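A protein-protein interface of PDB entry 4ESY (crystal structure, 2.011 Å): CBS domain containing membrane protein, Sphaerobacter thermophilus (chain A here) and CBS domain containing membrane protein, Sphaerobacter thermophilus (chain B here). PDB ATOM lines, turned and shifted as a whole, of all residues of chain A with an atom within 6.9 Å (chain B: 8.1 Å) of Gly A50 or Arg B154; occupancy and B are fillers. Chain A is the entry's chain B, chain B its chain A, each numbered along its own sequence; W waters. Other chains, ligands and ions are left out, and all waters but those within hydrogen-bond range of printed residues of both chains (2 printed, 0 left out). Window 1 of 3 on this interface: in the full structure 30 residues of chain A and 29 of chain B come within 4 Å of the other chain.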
ATOM      1  N   MET A  44     -13.443 -13.471 -22.211  1.00  0.00           N
ATOM      2  CA  MET A  44     -13.173 -14.632 -23.092  1.00  0.00           C
ATOM      3  C   MET A  44     -14.333 -15.615 -23.119  1.00  0.00           C
ATOM      4  O   MET A  44     -14.688 -16.157 -24.173  1.00  0.00           O
ATOM      5  CB  MET A  44     -11.913 -15.388 -22.640  1.00  0.00           C
ATOM      6  CG  MET A  44     -10.556 -14.671 -22.924  1.00  0.00           C
ATOM      7  SD  MET A  44      -9.154 -15.827 -22.107  1.00  0.00           S
ATOM      8  CE  MET A  44      -7.647 -15.102 -23.052  1.00  0.00           C
ATOM      9  N   HIS A  47     -17.431 -14.110 -24.955  1.00  0.00           N
ATOM     10  CA  HIS A  47     -17.256 -14.163 -26.404  1.00  0.00           C
ATOM     11  C   HIS A  47     -16.852 -15.519 -26.997  1.00  0.00           C
ATOM     12  O   HIS A  47     -16.645 -15.635 -28.212  1.00  0.00           O
ATOM     13  CB  HIS A  47     -16.276 -13.057 -26.830  1.00  0.00           C
ATOM     14  CG  HIS A  47     -16.780 -11.687 -26.522  1.00  0.00           C
ATOM     15  ND1 HIS A  47     -16.290 -10.920 -25.489  1.00  0.00           N
ATOM     16  CD2 HIS A  47     -17.767 -10.957 -27.091  1.00  0.00           C
ATOM     17  CE1 HIS A  47     -16.947  -9.774 -25.440  1.00  0.00           C
ATOM     18  NE2 HIS A  47     -17.847  -9.771 -26.406  1.00  0.00           N
ATOM     19  N   GLN A  48     -16.736 -16.524 -26.131  1.00  0.00           N
ATOM     20  CA  GLN A  48     -16.331 -17.882 -26.522  1.00  0.00           C
ATOM     21  C   GLN A  48     -15.000 -17.935 -27.282  1.00  0.00           C
ATOM     22  O   GLN A  48     -14.899 -18.563 -28.324  1.00  0.00           O
ATOM     23  CB  GLN A  48     -17.428 -18.591 -27.324  1.00  0.00           C
ATOM     24  CG  GLN A  48     -18.739 -18.729 -26.578  1.00  0.00           C
ATOM     25  CD  GLN A  48     -19.755 -19.496 -27.376  1.00  0.00           C
ATOM     26  OE1 GLN A  48     -19.644 -20.710 -27.526  1.00  0.00           O
ATOM     27  NE2 GLN A  48     -20.752 -18.792 -27.907  1.00  0.00           N
ATOM     28  N   ILE A  49     -13.975 -17.288 -26.748  1.00  0.00           N
ATOM     29  CA  ILE A  49     -12.677 -17.310 -27.389  1.00  0.00           C
ATOM     30  C   ILE A  49     -11.637 -17.768 -26.365  1.00  0.00           C
ATOM     31  O   ILE A  49     -11.811 -17.553 -25.166  1.00  0.00           O
ATOM     32  CB  ILE A  49     -12.307 -15.901 -27.902  1.00  0.00           C
ATOM     33  CG1 ILE A  49     -12.281 -14.928 -26.734  1.00  0.00           C
ATOM     34  CG2 ILE A  49     -13.327 -15.444 -28.945  1.00  0.00           C
ATOM     35  CD1 ILE A  49     -11.902 -13.538 -27.091  1.00  0.00           C
ATOM     36  N   GLY A  50     -10.561 -18.389 -26.838  1.00  0.00           N
ATOM     37  CA  GLY A  50      -9.533 -18.893 -25.947  1.00  0.00           C
ATOM     38  C   GLY A  50      -8.250 -18.073 -25.988  1.00  0.00           C
ATOM     39  O   GLY A  50      -7.302 -18.391 -25.277  1.00  0.00           O
ATOM     40  N   CSO A  51      -8.221 -17.034 -26.822  1.00  0.00           N
ATOM     41  CA  CSO A  51      -7.079 -16.144 -26.869  1.00  0.00           C
ATOM     42  CB  CSO A  51      -5.940 -16.698 -27.743  1.00  0.00           C
ATOM     43  SG  CSO A  51      -6.365 -17.053 -29.470  1.00  0.00           S
ATOM     44  C   CSO A  51      -7.514 -14.749 -27.320  1.00  0.00           C
ATOM     45  O   CSO A  51      -8.561 -14.603 -27.930  1.00  0.00           O
ATOM     46  OD  CSO A  51      -5.981 -18.752 -29.845  1.00  0.00           O
ATOM     47  N   ALA A  52      -6.716 -13.737 -26.996  1.00  0.00           N
ATOM     48  CA  ALA A  52      -7.060 -12.352 -27.320  1.00  0.00           C
ATOM     49  C   ALA A  52      -5.796 -11.503 -27.366  1.00  0.00           C
ATOM     50  O   ALA A  52      -4.884 -11.722 -26.574  1.00  0.00           O
ATOM     51  CB  ALA A  52      -8.001 -11.794 -26.244  1.00  0.00           C
ATOM     52  N   ILE A  65      -2.718 -13.094 -24.937  1.00  0.00           N
ATOM     53  CA  ILE A  65      -2.998 -13.876 -23.733  1.00  0.00           C
ATOM     54  C   ILE A  65      -3.963 -14.992 -24.126  1.00  0.00           C
ATOM     55  O   ILE A  65      -4.850 -14.782 -24.972  1.00  0.00           O
ATOM     56  CB  ILE A  65      -3.583 -12.947 -22.613  1.00  0.00           C
ATOM     57  CG1 ILE A  65      -3.717 -13.656 -21.246  1.00  0.00           C
ATOM     58  CG2 ILE A  65      -4.914 -12.343 -23.040  1.00  0.00           C
ATOM     59  CD1 ILE A  65      -4.178 -12.654 -20.084  1.00  0.00           C
ATOM     60  N   THR A  66      -3.753 -16.171 -23.540  1.00  0.00           N
ATOM     61  CA  THR A  66      -4.585 -17.343 -23.788  1.00  0.00           C
ATOM     62  C   THR A  66      -4.995 -17.968 -22.460  1.00  0.00           C
ATOM     63  O   THR A  66      -4.466 -17.595 -21.378  1.00  0.00           O
ATOM     64  CB  THR A  66      -3.794 -18.456 -24.475  1.00  0.00           C
ATOM     65  OG1 THR A  66      -2.756 -18.883 -23.576  1.00  0.00           O
ATOM     66  CG2 THR A  66      -3.194 -17.982 -25.798  1.00  0.00           C
ATOM     67  N   GLU A  67      -5.912 -18.926 -22.533  1.00  0.00           N
ATOM     68  CA  GLU A  67      -6.368 -19.596 -21.314  1.00  0.00           C
ATOM     69  C   GLU A  67      -5.204 -20.219 -20.555  1.00  0.00           C
ATOM     70  O   GLU A  67      -5.169 -20.131 -19.332  1.00  0.00           O
ATOM     71  CB  GLU A  67      -7.413 -20.653 -21.631  1.00  0.00           C
ATOM     72  CG  GLU A  67      -8.648 -20.093 -22.357  1.00  0.00           C
ATOM     73  CD  GLU A  67      -9.462 -21.195 -23.066  1.00  0.00           C
ATOM     74  OE1 GLU A  67      -8.884 -22.238 -23.446  1.00  0.00           O
ATOM     75  OE2 GLU A  67     -10.690 -21.014 -23.246  1.00  0.00           O
ATOM     76  N   SER A  68      -4.242 -20.799 -21.285  1.00  0.00           N
ATOM     77  CA  SER A  68      -3.162 -21.529 -20.655  1.00  0.00           C
ATOM     78  C   SER A  68      -2.249 -20.577 -19.894  1.00  0.00           C
ATOM     79  O   SER A  68      -1.604 -20.979 -18.923  1.00  0.00           O
ATOM     80  CB  SER A  68      -2.352 -22.332 -21.697  1.00  0.00           C
ATOM     81  OG  SER A  68      -1.868 -21.468 -22.711  1.00  0.00           O
ATOM     82  N   PHE A  77      -7.511 -21.868 -15.537  1.00  0.00           N
ATOM     83  CA  PHE A  77      -8.616 -21.133 -16.174  1.00  0.00           C
ATOM     84  C   PHE A  77      -9.982 -21.806 -15.918  1.00  0.00           C
ATOM     85  O   PHE A  77     -11.022 -21.140 -15.842  1.00  0.00           O
ATOM     86  CB  PHE A  77      -8.346 -20.965 -17.665  1.00  0.00           C
ATOM     87  CG  PHE A  77      -9.431 -20.211 -18.401  1.00  0.00           C
ATOM     88  CD1 PHE A  77      -9.325 -18.833 -18.606  1.00  0.00           C
ATOM     89  CD2 PHE A  77     -10.543 -20.865 -18.866  1.00  0.00           C
ATOM     90  CE1 PHE A  77     -10.333 -18.129 -19.296  1.00  0.00           C
ATOM     91  CE2 PHE A  77     -11.569 -20.156 -19.557  1.00  0.00           C
ATOM     92  CZ  PHE A  77     -11.448 -18.792 -19.757  1.00  0.00           C
ATOM     93  N   GLU A  81     -14.990 -21.509 -15.375  1.00  0.00           N
ATOM     94  CA  GLU A  81     -16.073 -22.231 -16.063  1.00  0.00           C
ATOM     95  C   GLU A  81     -16.822 -23.214 -15.180  1.00  0.00           C
ATOM     96  O   GLU A  81     -18.008 -23.455 -15.382  1.00  0.00           O
ATOM     97  CB  GLU A  81     -15.531 -23.037 -17.251  1.00  0.00           C
ATOM     98  CG  GLU A  81     -14.830 -22.224 -18.307  1.00  0.00           C
ATOM     99  CD  GLU A  81     -14.494 -23.045 -19.565  1.00  0.00           C
ATOM    100  OE1 GLU A  81     -13.328 -23.418 -19.732  1.00  0.00           O
ATOM    101  OE2 GLU A  81     -15.380 -23.307 -20.398  1.00  0.00           O
ATOM    102  N   ARG A 138       0.045 -19.245 -33.211  1.00  0.00           N
ATOM    103  CA  ARG A 138      -0.824 -18.072 -33.274  1.00  0.00           C
ATOM    104  C   ARG A 138      -0.034 -16.892 -33.777  1.00  0.00           C
ATOM    105  O   ARG A 138       1.069 -16.677 -33.309  1.00  0.00           O
ATOM    106  CB  ARG A 138      -1.270 -17.687 -31.867  1.00  0.00           C
ATOM    107  CG  ARG A 138      -2.592 -18.244 -31.446  1.00  0.00           C
ATOM    108  CD  ARG A 138      -2.819 -17.934 -29.973  1.00  0.00           C
ATOM    109  NE  ARG A 138      -2.030 -18.791 -29.108  1.00  0.00           N
ATOM    110  CZ  ARG A 138      -2.465 -19.947 -28.613  1.00  0.00           C
ATOM    111  NH1 ARG A 138      -3.687 -20.378 -28.909  1.00  0.00           N
ATOM    112  NH2 ARG A 138      -1.681 -20.666 -27.820  1.00  0.00           N
ATOM    113  N   ARG A 154      -5.114 -23.767 -36.358  1.00  0.00           N
ATOM    114  CA  ARG A 154      -6.410 -24.343 -36.720  1.00  0.00           C
ATOM    115  C   ARG A 154      -7.103 -23.631 -37.892  1.00  0.00           C
ATOM    116  O   ARG A 154      -7.648 -24.300 -38.779  1.00  0.00           O
ATOM    117  CB  ARG A 154      -7.374 -24.392 -35.522  1.00  0.00           C
ATOM    118  CG  ARG A 154      -8.817 -24.724 -35.976  1.00  0.00           C
ATOM    119  CD  ARG A 154      -9.850 -24.859 -34.835  1.00  0.00           C
ATOM    120  NE  ARG A 154     -11.178 -25.221 -35.344  1.00  0.00           N
ATOM    121  CZ  ARG A 154     -12.292 -25.190 -34.604  1.00  0.00           C
ATOM    122  NH1 ARG A 154     -12.228 -24.787 -33.327  1.00  0.00           N
ATOM    123  NH2 ARG A 154     -13.473 -25.536 -35.132  1.00  0.00           N
ATOM    124  N   MET B 131      -1.010 -37.744 -23.091  1.00  0.00           N
ATOM    125  CA  MET B 131      -0.955 -36.658 -24.072  1.00  0.00           C
ATOM    126  C   MET B 131       0.503 -36.276 -24.365  1.00  0.00           C
ATOM    127  O   MET B 131       0.949 -36.270 -25.518  1.00  0.00           O
ATOM    128  CB  MET B 131      -1.769 -35.469 -23.532  1.00  0.00           C
ATOM    129  CG  MET B 131      -2.146 -34.355 -24.507  1.00  0.00           C
ATOM    130  SD  MET B 131      -3.690 -34.656 -25.659  1.00  0.00           S
ATOM    131  CE  MET B 131      -5.168 -34.749 -24.388  1.00  0.00           C
ATOM    132  N   ILE B 136       0.668 -36.103 -28.559  1.00  0.00           N
ATOM    133  CA  ILE B 136      -0.515 -35.970 -29.405  1.00  0.00           C
ATOM    134  C   ILE B 136      -1.358 -34.812 -28.909  1.00  0.00           C
ATOM    135  O   ILE B 136      -0.977 -34.145 -27.956  1.00  0.00           O
ATOM    136  CB  ILE B 136      -1.333 -37.263 -29.478  1.00  0.00           C
ATOM    137  CG1 ILE B 136      -1.779 -37.703 -28.093  1.00  0.00           C
ATOM    138  CG2 ILE B 136      -0.491 -38.377 -30.096  1.00  0.00           C
ATOM    139  CD1 ILE B 136      -2.414 -39.070 -28.109  1.00  0.00           C
ATOM    140  N   HIS B 137      -2.480 -34.556 -29.568  1.00  0.00           N
ATOM    141  CA  HIS B 137      -3.263 -33.357 -29.296  1.00  0.00           C
ATOM    142  C   HIS B 137      -4.716 -33.665 -28.919  1.00  0.00           C
ATOM    143  O   HIS B 137      -5.445 -32.769 -28.474  1.00  0.00           O
ATOM    144  CB  HIS B 137      -3.250 -32.429 -30.501  1.00  0.00           C
ATOM    145  CG  HIS B 137      -1.934 -31.757 -30.733  1.00  0.00           C
ATOM    146  ND1 HIS B 137      -1.461 -30.743 -29.922  1.00  0.00           N
ATOM    147  CD2 HIS B 137      -0.992 -31.948 -31.686  1.00  0.00           C
ATOM    148  CE1 HIS B 137      -0.285 -30.339 -30.368  1.00  0.00           C
ATOM    149  NE2 HIS B 137       0.020 -31.050 -31.441  1.00  0.00           N
ATOM    150  N   ARG B 138      -5.128 -34.920 -29.114  1.00  0.00           N
ATOM    151  CA  ARG B 138      -6.503 -35.343 -28.844  1.00  0.00           C
ATOM    152  C   ARG B 138      -6.532 -36.803 -28.416  1.00  0.00           C
ATOM    153  O   ARG B 138      -5.811 -37.623 -28.975  1.00  0.00           O
ATOM    154  CB  ARG B 138      -7.342 -35.266 -30.121  1.00  0.00           C
ATOM    155  CG  ARG B 138      -7.626 -33.896 -30.625  1.00  0.00           C
ATOM    156  CD  ARG B 138      -8.141 -33.998 -32.054  1.00  0.00           C
ATOM    157  NE  ARG B 138      -7.934 -32.750 -32.766  1.00  0.00           N
ATOM    158  CZ  ARG B 138      -6.932 -32.552 -33.616  1.00  0.00           C
ATOM    159  NH1 ARG B 138      -6.060 -33.529 -33.857  1.00  0.00           N
ATOM    160  NH2 ARG B 138      -6.814 -31.386 -34.238  1.00  0.00           N
ATOM    161  N   VAL B 151     -10.922 -35.576 -25.486  1.00  0.00           N
ATOM    162  CA  VAL B 151     -10.175 -34.645 -24.670  1.00  0.00           C
ATOM    163  C   VAL B 151      -9.020 -34.055 -25.494  1.00  0.00           C
ATOM    164  O   VAL B 151      -8.251 -34.793 -26.104  1.00  0.00           O
ATOM    165  CB  VAL B 151      -9.602 -35.344 -23.457  1.00  0.00           C
ATOM    166  CG1 VAL B 151      -8.644 -34.396 -22.707  1.00  0.00           C
ATOM    167  CG2 VAL B 151     -10.755 -35.820 -22.545  1.00  0.00           C
ATOM    168  N   THR B 152      -8.912 -32.728 -25.518  1.00  0.00           N
ATOM    169  CA  THR B 152      -7.864 -32.062 -26.305  1.00  0.00           C
ATOM    170  C   THR B 152      -6.800 -31.448 -25.389  1.00  0.00           C
ATOM    171  O   THR B 152      -7.026 -31.243 -24.193  1.00  0.00           O
ATOM    172  CB  THR B 152      -8.444 -30.963 -27.217  1.00  0.00           C
ATOM    173  OG1 THR B 152      -9.060 -29.954 -26.405  1.00  0.00           O
ATOM    174  CG2 THR B 152      -9.525 -31.554 -28.151  1.00  0.00           C
ATOM    175  N   ARG B 153      -5.655 -31.123 -25.975  1.00  0.00           N
ATOM    176  CA  ARG B 153      -4.597 -30.456 -25.250  1.00  0.00           C
ATOM    177  C   ARG B 153      -5.141 -29.103 -24.751  1.00  0.00           C
ATOM    178  O   ARG B 153      -4.860 -28.707 -23.645  1.00  0.00           O
ATOM    179  CB  ARG B 153      -3.378 -30.341 -26.168  1.00  0.00           C
ATOM    180  CG  ARG B 153      -2.163 -29.696 -25.582  1.00  0.00           C
ATOM    181  CD  ARG B 153      -0.978 -29.786 -26.536  1.00  0.00           C
ATOM    182  NE  ARG B 153      -0.479 -31.158 -26.697  1.00  0.00           N
ATOM    183  CZ  ARG B 153       0.636 -31.635 -26.131  1.00  0.00           C
ATOM    184  NH1 ARG B 153       1.392 -30.852 -25.359  1.00  0.00           N
ATOM    185  NH2 ARG B 153       1.012 -32.893 -26.348  1.00  0.00           N
ATOM    186  N   ARG B 154      -5.983 -28.438 -25.533  1.00  0.00           N
ATOM    187  CA  ARG B 154      -6.575 -27.178 -25.099  1.00  0.00           C
ATOM    188  C   ARG B 154      -7.442 -27.344 -23.842  1.00  0.00           C
ATOM    189  O   ARG B 154      -7.362 -26.526 -22.929  1.00  0.00           O
ATOM    190  CB  ARG B 154      -7.427 -26.535 -26.214  1.00  0.00           C
ATOM    191  CG  ARG B 154      -8.304 -25.412 -25.648  1.00  0.00           C
ATOM    192  CD  ARG B 154      -9.203 -24.719 -26.655  1.00  0.00           C
ATOM    193  NE  ARG B 154      -9.901 -23.596 -26.022  1.00  0.00           N
ATOM    194  CZ  ARG B 154     -10.820 -22.842 -26.621  1.00  0.00           C
ATOM    195  NH1 ARG B 154     -11.180 -23.088 -27.887  1.00  0.00           N
ATOM    196  NH2 ARG B 154     -11.390 -21.838 -25.951  1.00  0.00           N
ATOM    197  N   ASP B 155      -8.286 -28.377 -23.817  1.00  0.00           N
ATOM    198  CA  ASP B 155      -9.044 -28.714 -22.611  1.00  0.00           C
ATOM    199  C   ASP B 155      -8.129 -28.835 -21.378  1.00  0.00           C
ATOM    200  O   ASP B 155      -8.443 -28.308 -20.315  1.00  0.00           O
ATOM    201  CB  ASP B 155      -9.785 -30.056 -22.740  1.00  0.00           C
ATOM    202  CG  ASP B 155     -10.868 -30.051 -23.827  1.00  0.00           C
ATOM    203  OD1 ASP B 155     -11.464 -28.969 -24.120  1.00  0.00           O
ATOM    204  OD2 ASP B 155     -11.125 -31.154 -24.383  1.00  0.00           O
ATOM    205  N   LEU B 156      -7.028 -29.564 -21.507  1.00  0.00           N
ATOM    206  CA  LEU B 156      -6.201 -29.840 -20.340  1.00  0.00           C
ATOM    207  C   LEU B 156      -5.424 -28.588 -19.903  1.00  0.00           C
ATOM    208  O   LEU B 156      -5.150 -28.412 -18.722  1.00  0.00           O
ATOM    209  CB  LEU B 156      -5.226 -30.976 -20.616  1.00  0.00           C
ATOM    210  CG  LEU B 156      -5.814 -32.373 -20.880  1.00  0.00           C
ATOM    211  CD1 LEU B 156      -4.698 -33.322 -21.079  1.00  0.00           C
ATOM    212  CD2 LEU B 156      -6.714 -32.875 -19.748  1.00  0.00           C
ATOM    213  N   LEU B 157      -5.104 -27.703 -20.848  1.00  0.00           N
ATOM    214  CA  LEU B 157      -4.315 -26.533 -20.483  1.00  0.00           C
ATOM    215  C   LEU B 157      -5.138 -25.568 -19.638  1.00  0.00           C
ATOM    216  O   LEU B 157      -4.602 -24.604 -19.099  1.00  0.00           O
ATOM    217  CB  LEU B 157      -3.782 -25.849 -21.731  1.00  0.00           C
ATOM    218  CG  LEU B 157      -2.649 -26.631 -22.373  1.00  0.00           C
ATOM    219  CD1 LEU B 157      -2.296 -26.053 -23.745  1.00  0.00           C
ATOM    220  CD2 LEU B 157      -1.424 -26.574 -21.468  1.00  0.00           C
ATOM    221  N   LYS B 158      -6.439 -25.821 -19.546  1.00  0.00           N
ATOM    222  CA  LYS B 158      -7.327 -25.072 -18.654  1.00  0.00           C
ATOM    223  C   LYS B 158      -7.180 -25.524 -17.182  1.00  0.00           C
ATOM    224  O   LYS B 158      -7.679 -24.870 -16.257  1.00  0.00           O
ATOM    225  CB  LYS B 158      -8.790 -25.261 -19.083  1.00  0.00           C
ATOM    226  CG  LYS B 158      -9.143 -24.570 -20.408  1.00  0.00           C
ATOM    227  CD  LYS B 158     -10.567 -24.888 -20.751  1.00  0.00           C
ATOM    228  CE  LYS B 158     -11.041 -24.034 -21.889  1.00  0.00           C
ATOM    229  NZ  LYS B 158     -12.390 -24.461 -22.273  1.00  0.00           N
ATOM    230  N   LEU B 159      -6.484 -26.631 -16.997  1.00  0.00           N
ATOM    231  CA  LEU B 159      -6.239 -27.244 -15.690  1.00  0.00           C
ATOM    232  C   LEU B 159      -4.797 -27.355 -15.269  1.00  0.00           C
ATOM    233  O   LEU B 159      -4.485 -27.193 -14.092  1.00  0.00           O
ATOM    234  CB  LEU B 159      -6.767 -28.684 -15.728  1.00  0.00           C
ATOM    235  CG  LEU B 159      -8.264 -28.769 -15.919  1.00  0.00           C
ATOM    236  CD1 LEU B 159      -8.624 -30.213 -16.250  1.00  0.00           C
ATOM    237  CD2 LEU B 159      -8.874 -28.329 -14.629  1.00  0.00           C
ATOM    238  N   LEU B 160      -3.894 -27.708 -16.177  1.00  0.00           N
ATOM    239  CA  LEU B 160      -2.518 -27.937 -15.714  1.00  0.00           C
ATOM    240  C   LEU B 160      -1.559 -27.797 -16.873  1.00  0.00           C
ATOM    241  O   LEU B 160      -1.971 -27.894 -18.031  1.00  0.00           O
ATOM    242  CB  LEU B 160      -2.363 -29.364 -15.095  1.00  0.00           C
ATOM    243  CG  LEU B 160      -2.351 -30.594 -16.022  1.00  0.00           C
ATOM    244  CD1 LEU B 160      -1.913 -31.868 -15.279  1.00  0.00           C
ATOM    245  CD2 LEU B 160      -3.690 -30.834 -16.655  1.00  0.00           C
ATOM    246  N   LEU B 162       1.410 -28.795 -19.475  1.00  0.00           N
ATOM    247  CA  LEU B 162       1.813 -30.014 -20.178  1.00  0.00           C
ATOM    248  C   LEU B 162       3.295 -29.952 -20.557  1.00  0.00           C
ATOM    249  O   LEU B 162       3.651 -29.488 -21.645  1.00  0.00           O
ATOM    250  CB  LEU B 162       0.962 -30.219 -21.432  1.00  0.00           C
ATOM    251  CG  LEU B 162      -0.528 -30.302 -21.151  1.00  0.00           C
ATOM    252  CD1 LEU B 162      -1.279 -30.479 -22.430  1.00  0.00           C
ATOM    253  CD2 LEU B 162      -0.798 -31.468 -20.229  1.00  0.00           C
HETATM  254  O   HOH W   1      -5.433 -22.375 -17.404  1.00  0.00           O
HETATM  255  O   HOH W   2      -6.579 -23.790 -22.831  1.00  0.00           O
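The guanidinium group of Arg B154 is in salt-bridge range of the side-chain carboxylate of Glu A67 (2.9 Å). OE1 of Glu A81 lies within salt-bridge range of NZ of Lys B158, 2.9 Å away. O of Lys B158 lies within hydrogen-bond range of N of Phe A77. OE2 of Glu A67 lies within salt-bridge range of NZ of Lys B158.
N of Glu A67 sits at hydrogen-bond distance from O of Gly A50. The side-chain hydroxyl (OG1) of Thr A66 sits at hydrogen-bond distance from the side-chain hydroxyl (OG) of Ser A68 (2.9 Å).
Arg B154 touches Gly A50 (NH2 to CA, 3.5 Å). Leu B157 touches Ser A68 (O to CA, 3.7 Å).
Gly A50 touches just one residue of chain B: Arg B154 (3.5 Å). Of chain A, only Gly A50 and Glu A67 come within 4 Å of Arg B154. Of the printed residues of chain B, Glu A81 touches Lys B158. Printed residues of chain B within 4 Å of Glu A67: Arg B154 (2.9 Å) and Lys B158 (3.2 Å). Of the printed residues of chain A, Lys B158 touches Glu A67, Phe A77 and Glu A81. Of the printed residues of chain B, Phe A77 touches Lys B158. CSO A51 touches none of the printed residues of chain B. The nearest residue of chain B that does not touch Gly A50 is Lys B158 (6.7 Å). The nearest residue of chain A that does not touch Arg B154 is Ile A49 (4.1 Å).
Of the 15 printed residues of chain A, 5 touch a printed residue of chain B. Of the 15 printed residues of chain B, 3 touch a printed residue of chain A. Printed residues of chain B that touch a printed residue of chain A: Arg B154, Leu B157 and Lys B158. Hydrophobic or aromatic side chains of chain B within 4 Å of the printed part of chain A: Leu B157.
Water W1 lies within hydrogen-bond range of N of Phe A77 (2.8 Å), O of Leu B157 (2.9 Å) and O of Glu A67 (3.0 Å). Water W2 bridges OE1 of Glu A67 (2.8 Å) and O of Arg B154 (2.8 Å).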
